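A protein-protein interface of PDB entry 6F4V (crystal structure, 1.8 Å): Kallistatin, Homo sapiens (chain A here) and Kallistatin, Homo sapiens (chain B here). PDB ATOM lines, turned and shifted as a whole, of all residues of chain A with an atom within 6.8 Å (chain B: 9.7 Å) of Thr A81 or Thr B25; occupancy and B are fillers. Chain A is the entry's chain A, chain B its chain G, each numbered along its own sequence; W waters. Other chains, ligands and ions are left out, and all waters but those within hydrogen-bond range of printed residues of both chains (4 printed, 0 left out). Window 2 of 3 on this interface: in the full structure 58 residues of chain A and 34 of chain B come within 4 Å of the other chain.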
ATOM      1  N   SER A   2      -8.827 -22.745  30.467  1.00  0.00           N
ATOM      2  CA  SER A   2      -9.512 -23.075  29.223  1.00  0.00           C
ATOM      3  C   SER A   2     -10.730 -23.956  29.544  1.00  0.00           C
ATOM      4  O   SER A   2     -11.366 -24.528  28.638  1.00  0.00           O
ATOM      5  CB  SER A   2      -8.577 -23.838  28.309  1.00  0.00           C
ATOM      6  OG  SER A   2      -8.036 -25.003  28.939  1.00  0.00           O
ATOM      7  N   LEU A   3     -11.072 -24.042  30.833  1.00  0.00           N
ATOM      8  CA  LEU A   3     -12.255 -24.766  31.256  1.00  0.00           C
ATOM      9  C   LEU A   3     -13.546 -24.106  30.796  1.00  0.00           C
ATOM     10  O   LEU A   3     -14.521 -24.814  30.578  1.00  0.00           O
ATOM     11  CB  LEU A   3     -12.255 -24.990  32.769  1.00  0.00           C
ATOM     12  CG  LEU A   3     -11.420 -26.194  33.261  1.00  0.00           C
ATOM     13  CD1 LEU A   3     -10.247 -26.612  32.364  1.00  0.00           C
ATOM     14  CD2 LEU A   3     -10.935 -25.926  34.683  1.00  0.00           C
ATOM     15  N   ILE A   5     -14.218 -23.020  27.861  1.00  0.00           N
ATOM     16  CA  ILE A   5     -14.528 -23.447  26.489  1.00  0.00           C
ATOM     17  C   ILE A   5     -14.695 -24.957  26.345  1.00  0.00           C
ATOM     18  O   ILE A   5     -15.035 -25.422  25.264  1.00  0.00           O
ATOM     19  CB  ILE A   5     -13.522 -22.893  25.454  1.00  0.00           C
ATOM     20  CG1 ILE A   5     -12.109 -23.417  25.641  1.00  0.00           C
ATOM     21  CG2 ILE A   5     -13.558 -21.350  25.498  1.00  0.00           C
ATOM     22  CD1 ILE A   5     -11.226 -23.105  24.459  1.00  0.00           C
ATOM     23  N   ALA A   6     -14.452 -25.710  27.422  1.00  0.00           N
ATOM     24  CA  ALA A   6     -14.458 -27.177  27.343  1.00  0.00           C
ATOM     25  C   ALA A   6     -15.847 -27.718  26.963  1.00  0.00           C
ATOM     26  O   ALA A   6     -15.921 -28.605  26.122  1.00  0.00           O
ATOM     27  CB  ALA A   6     -13.953 -27.808  28.630  1.00  0.00           C
ATOM     28  N   LEU A  34     -10.667 -30.694  18.136  1.00  0.00           N
ATOM     29  CA  LEU A  34      -9.914 -29.548  18.602  1.00  0.00           C
ATOM     30  C   LEU A  34      -9.304 -28.761  17.445  1.00  0.00           C
ATOM     31  O   LEU A  34      -9.376 -27.537  17.404  1.00  0.00           O
ATOM     32  CB  LEU A  34      -8.846 -29.992  19.627  1.00  0.00           C
ATOM     33  CG  LEU A  34      -8.004 -28.806  20.104  1.00  0.00           C
ATOM     34  CD1 LEU A  34      -8.885 -27.781  20.790  1.00  0.00           C
ATOM     35  CD2 LEU A  34      -6.911 -29.238  20.999  1.00  0.00           C
ATOM     36  N   PHE A  75      -8.997 -20.448  24.209  1.00  0.00           N
ATOM     37  CA  PHE A  75      -8.153 -21.159  23.221  1.00  0.00           C
ATOM     38  C   PHE A  75      -6.672 -20.867  23.434  1.00  0.00           C
ATOM     39  O   PHE A  75      -5.859 -21.758  23.345  1.00  0.00           O
ATOM     40  CB  PHE A  75      -8.553 -20.839  21.771  1.00  0.00           C
ATOM     41  CG  PHE A  75      -9.713 -21.661  21.277  1.00  0.00           C
ATOM     42  CD1 PHE A  75      -9.522 -23.012  20.935  1.00  0.00           C
ATOM     43  CD2 PHE A  75     -10.965 -21.135  21.164  1.00  0.00           C
ATOM     44  CE1 PHE A  75     -10.567 -23.795  20.486  1.00  0.00           C
ATOM     45  CE2 PHE A  75     -12.028 -21.915  20.699  1.00  0.00           C
ATOM     46  CZ  PHE A  75     -11.818 -23.254  20.368  1.00  0.00           C
ATOM     47  N   GLN A  76      -6.332 -19.611  23.695  1.00  0.00           N
ATOM     48  CA  GLN A  76      -4.941 -19.242  23.942  1.00  0.00           C
ATOM     49  C   GLN A  76      -4.368 -20.087  25.071  1.00  0.00           C
ATOM     50  O   GLN A  76      -3.274 -20.625  24.953  1.00  0.00           O
ATOM     51  CB  GLN A  76      -4.823 -17.758  24.318  1.00  0.00           C
ATOM     52  CG  GLN A  76      -3.372 -17.294  24.469  1.00  0.00           C
ATOM     53  CD  GLN A  76      -3.263 -15.868  24.967  1.00  0.00           C
ATOM     54  OE1 GLN A  76      -4.251 -15.262  25.370  1.00  0.00           O
ATOM     55  NE2 GLN A  76      -2.070 -15.317  24.917  1.00  0.00           N
ATOM     56  N   HIS A  77      -5.114 -20.194  26.160  1.00  0.00           N
ATOM     57  CA  HIS A  77      -4.672 -20.982  27.321  1.00  0.00           C
ATOM     58  C   HIS A  77      -4.639 -22.484  27.012  1.00  0.00           C
ATOM     59  O   HIS A  77      -3.752 -23.173  27.462  1.00  0.00           O
ATOM     60  CB  HIS A  77      -5.582 -20.737  28.533  1.00  0.00           C
ATOM     61  CG  HIS A  77      -5.147 -21.448  29.779  1.00  0.00           C
ATOM     62  ND1 HIS A  77      -5.701 -22.651  30.185  1.00  0.00           N
ATOM     63  CD2 HIS A  77      -4.207 -21.140  30.714  1.00  0.00           C
ATOM     64  CE1 HIS A  77      -5.115 -23.057  31.303  1.00  0.00           C
ATOM     65  NE2 HIS A  77      -4.212 -22.153  31.650  1.00  0.00           N
ATOM     66  N   LEU A  78      -5.646 -22.968  26.278  1.00  0.00           N
ATOM     67  CA  LEU A  78      -5.730 -24.369  25.860  1.00  0.00           C
ATOM     68  C   LEU A  78      -4.511 -24.766  25.038  1.00  0.00           C
ATOM     69  O   LEU A  78      -3.836 -25.755  25.333  1.00  0.00           O
ATOM     70  CB  LEU A  78      -7.010 -24.563  25.043  1.00  0.00           C
ATOM     71  CG  LEU A  78      -7.301 -25.820  24.226  1.00  0.00           C
ATOM     72  CD1 LEU A  78      -6.982 -27.021  25.048  1.00  0.00           C
ATOM     73  CD2 LEU A  78      -8.763 -25.838  23.832  1.00  0.00           C
ATOM     74  N   LEU A  79      -4.211 -23.961  24.028  1.00  0.00           N
ATOM     75  CA  LEU A  79      -3.100 -24.239  23.116  1.00  0.00           C
ATOM     76  C   LEU A  79      -1.734 -24.114  23.820  1.00  0.00           C
ATOM     77  O   LEU A  79      -0.835 -24.957  23.611  1.00  0.00           O
ATOM     78  CB  LEU A  79      -3.208 -23.339  21.890  1.00  0.00           C
ATOM     79  CG  LEU A  79      -4.520 -23.594  21.119  1.00  0.00           C
ATOM     80  CD1 LEU A  79      -4.760 -22.518  20.072  1.00  0.00           C
ATOM     81  CD2 LEU A  79      -4.525 -24.975  20.500  1.00  0.00           C
ATOM     82  N   HIS A  80      -1.611 -23.125  24.694  1.00  0.00           N
ATOM     83  CA  HIS A  80      -0.401 -22.963  25.524  1.00  0.00           C
ATOM     84  C   HIS A  80      -0.144 -24.212  26.366  1.00  0.00           C
ATOM     85  O   HIS A  80       0.975 -24.766  26.345  1.00  0.00           O
ATOM     86  CB  HIS A  80      -0.499 -21.709  26.405  1.00  0.00           C
ATOM     87  CG  HIS A  80       0.706 -21.499  27.274  1.00  0.00           C
ATOM     88  ND1 HIS A  80       1.859 -20.897  26.812  1.00  0.00           N
ATOM     89  CD2 HIS A  80       0.956 -21.860  28.557  1.00  0.00           C
ATOM     90  CE1 HIS A  80       2.759 -20.872  27.783  1.00  0.00           C
ATOM     91  NE2 HIS A  80       2.235 -21.452  28.849  1.00  0.00           N
ATOM     92  N   THR A  81      -1.173 -24.653  27.094  1.00  0.00           N
ATOM     93  CA  THR A  81      -1.104 -25.836  27.944  1.00  0.00           C
ATOM     94  C   THR A  81      -0.696 -27.066  27.116  1.00  0.00           C
ATOM     95  O   THR A  81       0.268 -27.770  27.481  1.00  0.00           O
ATOM     96  CB  THR A  81      -2.431 -26.064  28.707  1.00  0.00           C
ATOM     97  OG1 THR A  81      -2.701 -24.919  29.503  1.00  0.00           O
ATOM     98  CG2 THR A  81      -2.411 -27.288  29.613  1.00  0.00           C
ATOM     99  N   LEU A  82      -1.357 -27.301  25.982  1.00  0.00           N
ATOM    100  CA  LEU A  82      -0.981 -28.462  25.161  1.00  0.00           C
ATOM    101  C   LEU A  82       0.457 -28.400  24.674  1.00  0.00           C
ATOM    102  O   LEU A  82       1.133 -29.437  24.599  1.00  0.00           O
ATOM    103  CB  LEU A  82      -1.934 -28.623  23.968  1.00  0.00           C
ATOM    104  CG  LEU A  82      -3.362 -28.989  24.334  1.00  0.00           C
ATOM    105  CD1 LEU A  82      -4.201 -29.116  23.051  1.00  0.00           C
ATOM    106  CD2 LEU A  82      -3.391 -30.287  25.140  1.00  0.00           C
ATOM    107  N   ASN A  83       0.938 -27.208  24.351  1.00  0.00           N
ATOM    108  CA  ASN A  83       2.277 -27.075  23.821  1.00  0.00           C
ATOM    109  C   ASN A  83       3.392 -27.149  24.883  1.00  0.00           C
ATOM    110  O   ASN A  83       4.558 -27.158  24.519  1.00  0.00           O
ATOM    111  CB  ASN A  83       2.401 -25.786  23.004  1.00  0.00           C
ATOM    112  CG  ASN A  83       1.766 -25.921  21.643  1.00  0.00           C
ATOM    113  OD1 ASN A  83       1.900 -26.963  21.016  1.00  0.00           O
ATOM    114  ND2 ASN A  83       1.047 -24.895  21.190  1.00  0.00           N
ATOM    115  N   LEU A  84       3.052 -27.222  26.162  1.00  0.00           N
ATOM    116  CA  LEU A  84       4.087 -27.282  27.217  1.00  0.00           C
ATOM    117  C   LEU A  84       4.746 -28.661  27.258  1.00  0.00           C
ATOM    118  O   LEU A  84       4.066 -29.675  27.054  1.00  0.00           O
ATOM    119  CB  LEU A  84       3.507 -26.988  28.597  1.00  0.00           C
ATOM    120  CG  LEU A  84       3.161 -25.535  28.895  1.00  0.00           C
ATOM    121  CD1 LEU A  84       2.496 -25.444  30.266  1.00  0.00           C
ATOM    122  CD2 LEU A  84       4.382 -24.621  28.793  1.00  0.00           C
ATOM    123  N   PRO A  85       6.065 -28.704  27.553  1.00  0.00           N
ATOM    124  CA  PRO A  85       6.820 -29.957  27.741  1.00  0.00           C
ATOM    125  C   PRO A  85       6.110 -31.052  28.565  1.00  0.00           C
ATOM    126  O   PRO A  85       5.425 -30.745  29.544  1.00  0.00           O
ATOM    127  CB  PRO A  85       8.057 -29.484  28.497  1.00  0.00           C
ATOM    128  CG  PRO A  85       8.292 -28.093  28.009  1.00  0.00           C
ATOM    129  CD  PRO A  85       6.949 -27.521  27.657  1.00  0.00           C
ATOM    130  N   THR A  91       2.667 -33.324  22.536  1.00  0.00           N
ATOM    131  CA  THR A  91       1.554 -32.689  21.887  1.00  0.00           C
ATOM    132  C   THR A  91       2.049 -31.350  21.354  1.00  0.00           C
ATOM    133  O   THR A  91       2.731 -30.586  22.071  1.00  0.00           O
ATOM    134  CB  THR A  91       0.355 -32.522  22.834  1.00  0.00           C
ATOM    135  OG1 THR A  91       0.021 -33.793  23.389  1.00  0.00           O
ATOM    136  CG2 THR A  91      -0.837 -31.985  22.092  1.00  0.00           C
ATOM    137  N   ASP A 227      -0.542 -36.057  30.320  1.00  0.00           N
ATOM    138  CA  ASP A 227      -1.881 -35.638  30.697  1.00  0.00           C
ATOM    139  C   ASP A 227      -2.864 -35.982  29.580  1.00  0.00           C
ATOM    140  O   ASP A 227      -3.483 -35.074  28.988  1.00  0.00           O
ATOM    141  CB  ASP A 227      -1.895 -34.152  31.004  1.00  0.00           C
ATOM    142  CG  ASP A 227      -1.040 -33.802  32.223  1.00  0.00           C
ATOM    143  OD1 ASP A 227      -0.905 -34.652  33.117  1.00  0.00           O
ATOM    144  OD2 ASP A 227      -0.541 -32.660  32.289  1.00  0.00           O
ATOM    145  N   ILE B  20      -9.728 -39.781  22.283  1.00  0.00           N
ATOM    146  CA  ILE B  20      -8.448 -39.378  22.890  1.00  0.00           C
ATOM    147  C   ILE B  20      -8.704 -38.038  23.554  1.00  0.00           C
ATOM    148  O   ILE B  20      -9.103 -37.063  22.895  1.00  0.00           O
ATOM    149  CB  ILE B  20      -7.299 -39.282  21.859  1.00  0.00           C
ATOM    150  CG1 ILE B  20      -7.032 -40.644  21.233  1.00  0.00           C
ATOM    151  CG2 ILE B  20      -6.008 -38.776  22.508  1.00  0.00           C
ATOM    152  CD1 ILE B  20      -6.088 -40.584  20.065  1.00  0.00           C
ATOM    153  N   PHE B  21      -8.430 -38.000  24.856  1.00  0.00           N
ATOM    154  CA  PHE B  21      -8.824 -36.923  25.729  1.00  0.00           C
ATOM    155  C   PHE B  21      -7.612 -36.320  26.453  1.00  0.00           C
ATOM    156  O   PHE B  21      -6.810 -37.072  27.010  1.00  0.00           O
ATOM    157  CB  PHE B  21      -9.837 -37.533  26.714  1.00  0.00           C
ATOM    158  CG  PHE B  21     -10.565 -36.537  27.548  1.00  0.00           C
ATOM    159  CD1 PHE B  21     -11.481 -35.653  26.972  1.00  0.00           C
ATOM    160  CD2 PHE B  21     -10.365 -36.496  28.944  1.00  0.00           C
ATOM    161  CE1 PHE B  21     -12.157 -34.738  27.763  1.00  0.00           C
ATOM    162  CE2 PHE B  21     -11.069 -35.570  29.741  1.00  0.00           C
ATOM    163  CZ  PHE B  21     -11.947 -34.691  29.146  1.00  0.00           C
ATOM    164  N   SER B  22      -7.441 -34.986  26.379  1.00  0.00           N
ATOM    165  CA  SER B  22      -6.483 -34.246  27.202  1.00  0.00           C
ATOM    166  C   SER B  22      -7.073 -34.048  28.584  1.00  0.00           C
ATOM    167  O   SER B  22      -8.123 -33.408  28.747  1.00  0.00           O
ATOM    168  CB  SER B  22      -6.120 -32.891  26.586  1.00  0.00           C
ATOM    169  OG  SER B  22      -5.479 -32.038  27.524  1.00  0.00           O
ATOM    170  N   THR B  23      -6.417 -34.598  29.613  1.00  0.00           N
ATOM    171  CA  THR B  23      -6.948 -34.449  30.949  1.00  0.00           C
ATOM    172  C   THR B  23      -6.565 -33.085  31.546  1.00  0.00           C
ATOM    173  O   THR B  23      -7.267 -32.625  32.415  1.00  0.00           O
ATOM    174  CB  THR B  23      -6.502 -35.560  31.903  1.00  0.00           C
ATOM    175  OG1 THR B  23      -5.071 -35.548  31.962  1.00  0.00           O
ATOM    176  CG2 THR B  23      -6.961 -36.905  31.380  1.00  0.00           C
ATOM    177  N   SER B  24      -5.513 -32.436  31.066  1.00  0.00           N
ATOM    178  CA  SER B  24      -5.161 -31.093  31.555  1.00  0.00           C
ATOM    179  C   SER B  24      -6.106 -30.011  31.007  1.00  0.00           C
ATOM    180  O   SER B  24      -6.386 -29.037  31.697  1.00  0.00           O
ATOM    181  CB  SER B  24      -3.735 -30.735  31.205  1.00  0.00           C
ATOM    182  OG  SER B  24      -3.528 -30.859  29.818  1.00  0.00           O
ATOM    183  N   THR B  25      -6.587 -30.163  29.774  1.00  0.00           N
ATOM    184  CA  THR B  25      -7.478 -29.162  29.197  1.00  0.00           C
ATOM    185  C   THR B  25      -8.936 -29.611  29.089  1.00  0.00           C
ATOM    186  O   THR B  25      -9.803 -28.803  28.710  1.00  0.00           O
ATOM    187  CB  THR B  25      -7.004 -28.744  27.812  1.00  0.00           C
ATOM    188  OG1 THR B  25      -7.059 -29.854  26.912  1.00  0.00           O
ATOM    189  CG2 THR B  25      -5.570 -28.188  27.872  1.00  0.00           C
ATOM    190  N   GLN B  26      -9.210 -30.883  29.406  1.00  0.00           N
ATOM    191  CA  GLN B  26     -10.517 -31.490  29.290  1.00  0.00           C
ATOM    192  C   GLN B  26     -11.064 -31.403  27.833  1.00  0.00           C
ATOM    193  O   GLN B  26     -12.253 -31.138  27.638  1.00  0.00           O
ATOM    194  CB  GLN B  26     -11.498 -30.862  30.295  1.00  0.00           C
ATOM    195  CG  GLN B  26     -11.097 -31.041  31.759  1.00  0.00           C
ATOM    196  CD  GLN B  26     -11.214 -32.493  32.183  1.00  0.00           C
ATOM    197  OE1 GLN B  26     -10.206 -33.178  32.444  1.00  0.00           O
ATOM    198  NE2 GLN B  26     -12.436 -32.990  32.216  1.00  0.00           N
ATOM    199  N   SER B  27     -10.172 -31.572  26.858  1.00  0.00           N
ATOM    200  CA  SER B  27     -10.492 -31.487  25.429  1.00  0.00           C
ATOM    201  C   SER B  27     -10.445 -32.840  24.785  1.00  0.00           C
ATOM    202  O   SER B  27      -9.537 -33.647  25.034  1.00  0.00           O
ATOM    203  CB  SER B  27      -9.511 -30.624  24.649  1.00  0.00           C
ATOM    204  OG  SER B  27      -9.375 -29.419  25.312  1.00  0.00           O
ATOM    205  N   VAL B  28     -11.415 -33.071  23.928  1.00  0.00           N
ATOM    206  CA  VAL B  28     -11.362 -34.183  23.001  1.00  0.00           C
ATOM    207  C   VAL B  28     -10.424 -33.796  21.891  1.00  0.00           C
ATOM    208  O   VAL B  28     -10.738 -32.967  21.051  1.00  0.00           O
ATOM    209  CB  VAL B  28     -12.753 -34.556  22.432  1.00  0.00           C
ATOM    210  CG1 VAL B  28     -12.625 -35.747  21.484  1.00  0.00           C
ATOM    211  CG2 VAL B  28     -13.716 -34.902  23.574  1.00  0.00           C
ATOM    212  N   LEU B  29      -9.238 -34.396  21.905  1.00  0.00           N
ATOM    213  CA  LEU B  29      -8.250 -34.166  20.871  1.00  0.00           C
ATOM    214  C   LEU B  29      -8.548 -34.892  19.585  1.00  0.00           C
ATOM    215  O   LEU B  29      -8.341 -34.345  18.510  1.00  0.00           O
ATOM    216  CB  LEU B  29      -6.857 -34.526  21.366  1.00  0.00           C
ATOM    217  CG  LEU B  29      -6.393 -33.901  22.681  1.00  0.00           C
ATOM    218  CD1 LEU B  29      -5.017 -34.431  23.054  1.00  0.00           C
ATOM    219  CD2 LEU B  29      -6.364 -32.384  22.647  1.00  0.00           C
HETATM  220  O   HOH W   1     -10.779 -26.735  27.419  1.00  0.00           O
HETATM  221  O   HOH W   2      -3.087 -33.077  27.035  1.00  0.00           O
HETATM  222  O   HOH W   3     -11.995 -30.481  21.311  1.00  0.00           O
HETATM  223  O   HOH W   4     -13.673 -29.899  25.678  1.00  0.00           O
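The backbone NH (N) of Thr B23 is in hydrogen-bond range of the backbone carbonyl oxygen (O) of Asp A227, at 3.0 Å.
Water W1 lies within hydrogen-bond range of O of Ser A2 (2.6 Å) and O of Thr B25 (2.6 Å).
Water W4 lies within hydrogen-bond range of the backbone carbonyl oxygen (O) of Ala A6 (2.6 Å) and the backbone carbonyl oxygen (O) of Gln B26 (2.7 Å).
Water W2 lies within hydrogen-bond range of OG of Ser B22 (2.7 Å) and O of Asp A227 (2.8 Å).
Water W3 lies within hydrogen-bond range of the backbone carbonyl oxygen (O) of Val B28 (2.8 Å) and the backbone NH (N) of Leu A34 (3.4 Å).
Of chain B, only Ser B24 (3.7 Å) and Thr B25 (3.7 Å) come within 4 Å of Thr A81.
Of the printed residues of chain A, Thr B25 touches Leu A78 and Thr A81.
No residue of chain B comes within 4 Å of His A80.
No residue of chain B comes within 4 Å of Leu A84.
Of the printed residues of chain A, Leu B29 touches Leu A34 (3.6 Å) and Leu A82 (3.9 Å).
Printed residues of chain B within 4 Å of Asp A227: Ser B22 (3.6 Å), Thr B23 (3.0 Å) and Ser B24 (3.9 Å).
Of the printed residues of chain B, Leu A78 touches Thr B25 (3.3 Å) and Ser B27 (3.4 Å).
The nearest printed residue of chain A that does not touch Thr B25 is Ser A2 (4.04 Å).
Hydrophobic or aromatic side chains of chain A within 4 Å of the printed part of chain B: Ala A6, Leu A34, Leu A78 and Leu A82.
Among the printed residues, no Asp or Glu carboxylate lies within 4 Å of a Lys or Arg side-chain nitrogen of the other chain.
OG1 of Thr A81 lies within hydrogen-bond range of O of His A77 (2.9 Å).
The side-chain hydroxyl (OG) of Ser B24 is in hydrogen-bond range of the side-chain hydroxyl (OG) of Ser B22, 3.2 Å away.
OG of Ser B22 sits at hydrogen-bond distance from OG1 of Thr B25, 2.8 Å away.
The backbone NH (N) of Ser B22 is in hydrogen-bond range of the backbone carbonyl oxygen (O) of Ser B27 (2.8 Å).
O of Thr B23 sits close to OE1 of Gln B26 (3.0 Å).
OG1 of Thr B25 is in hydrogen-bond range of OG of Ser B27.
Among the printed residues, merely in contact across the chains: Leu A78 with Thr B25, Leu A78 with Ser B27, Asp A227 with Ser B22, Leu A34 with Leu B29, Leu A82 with Ser B22, Leu A34 with Val B28, Thr A81 with Thr B25, Thr A81 with Ser B24, Asp A227 with Ser B24, Ala A6 with Gln B26 and Leu A82 with Leu B29.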
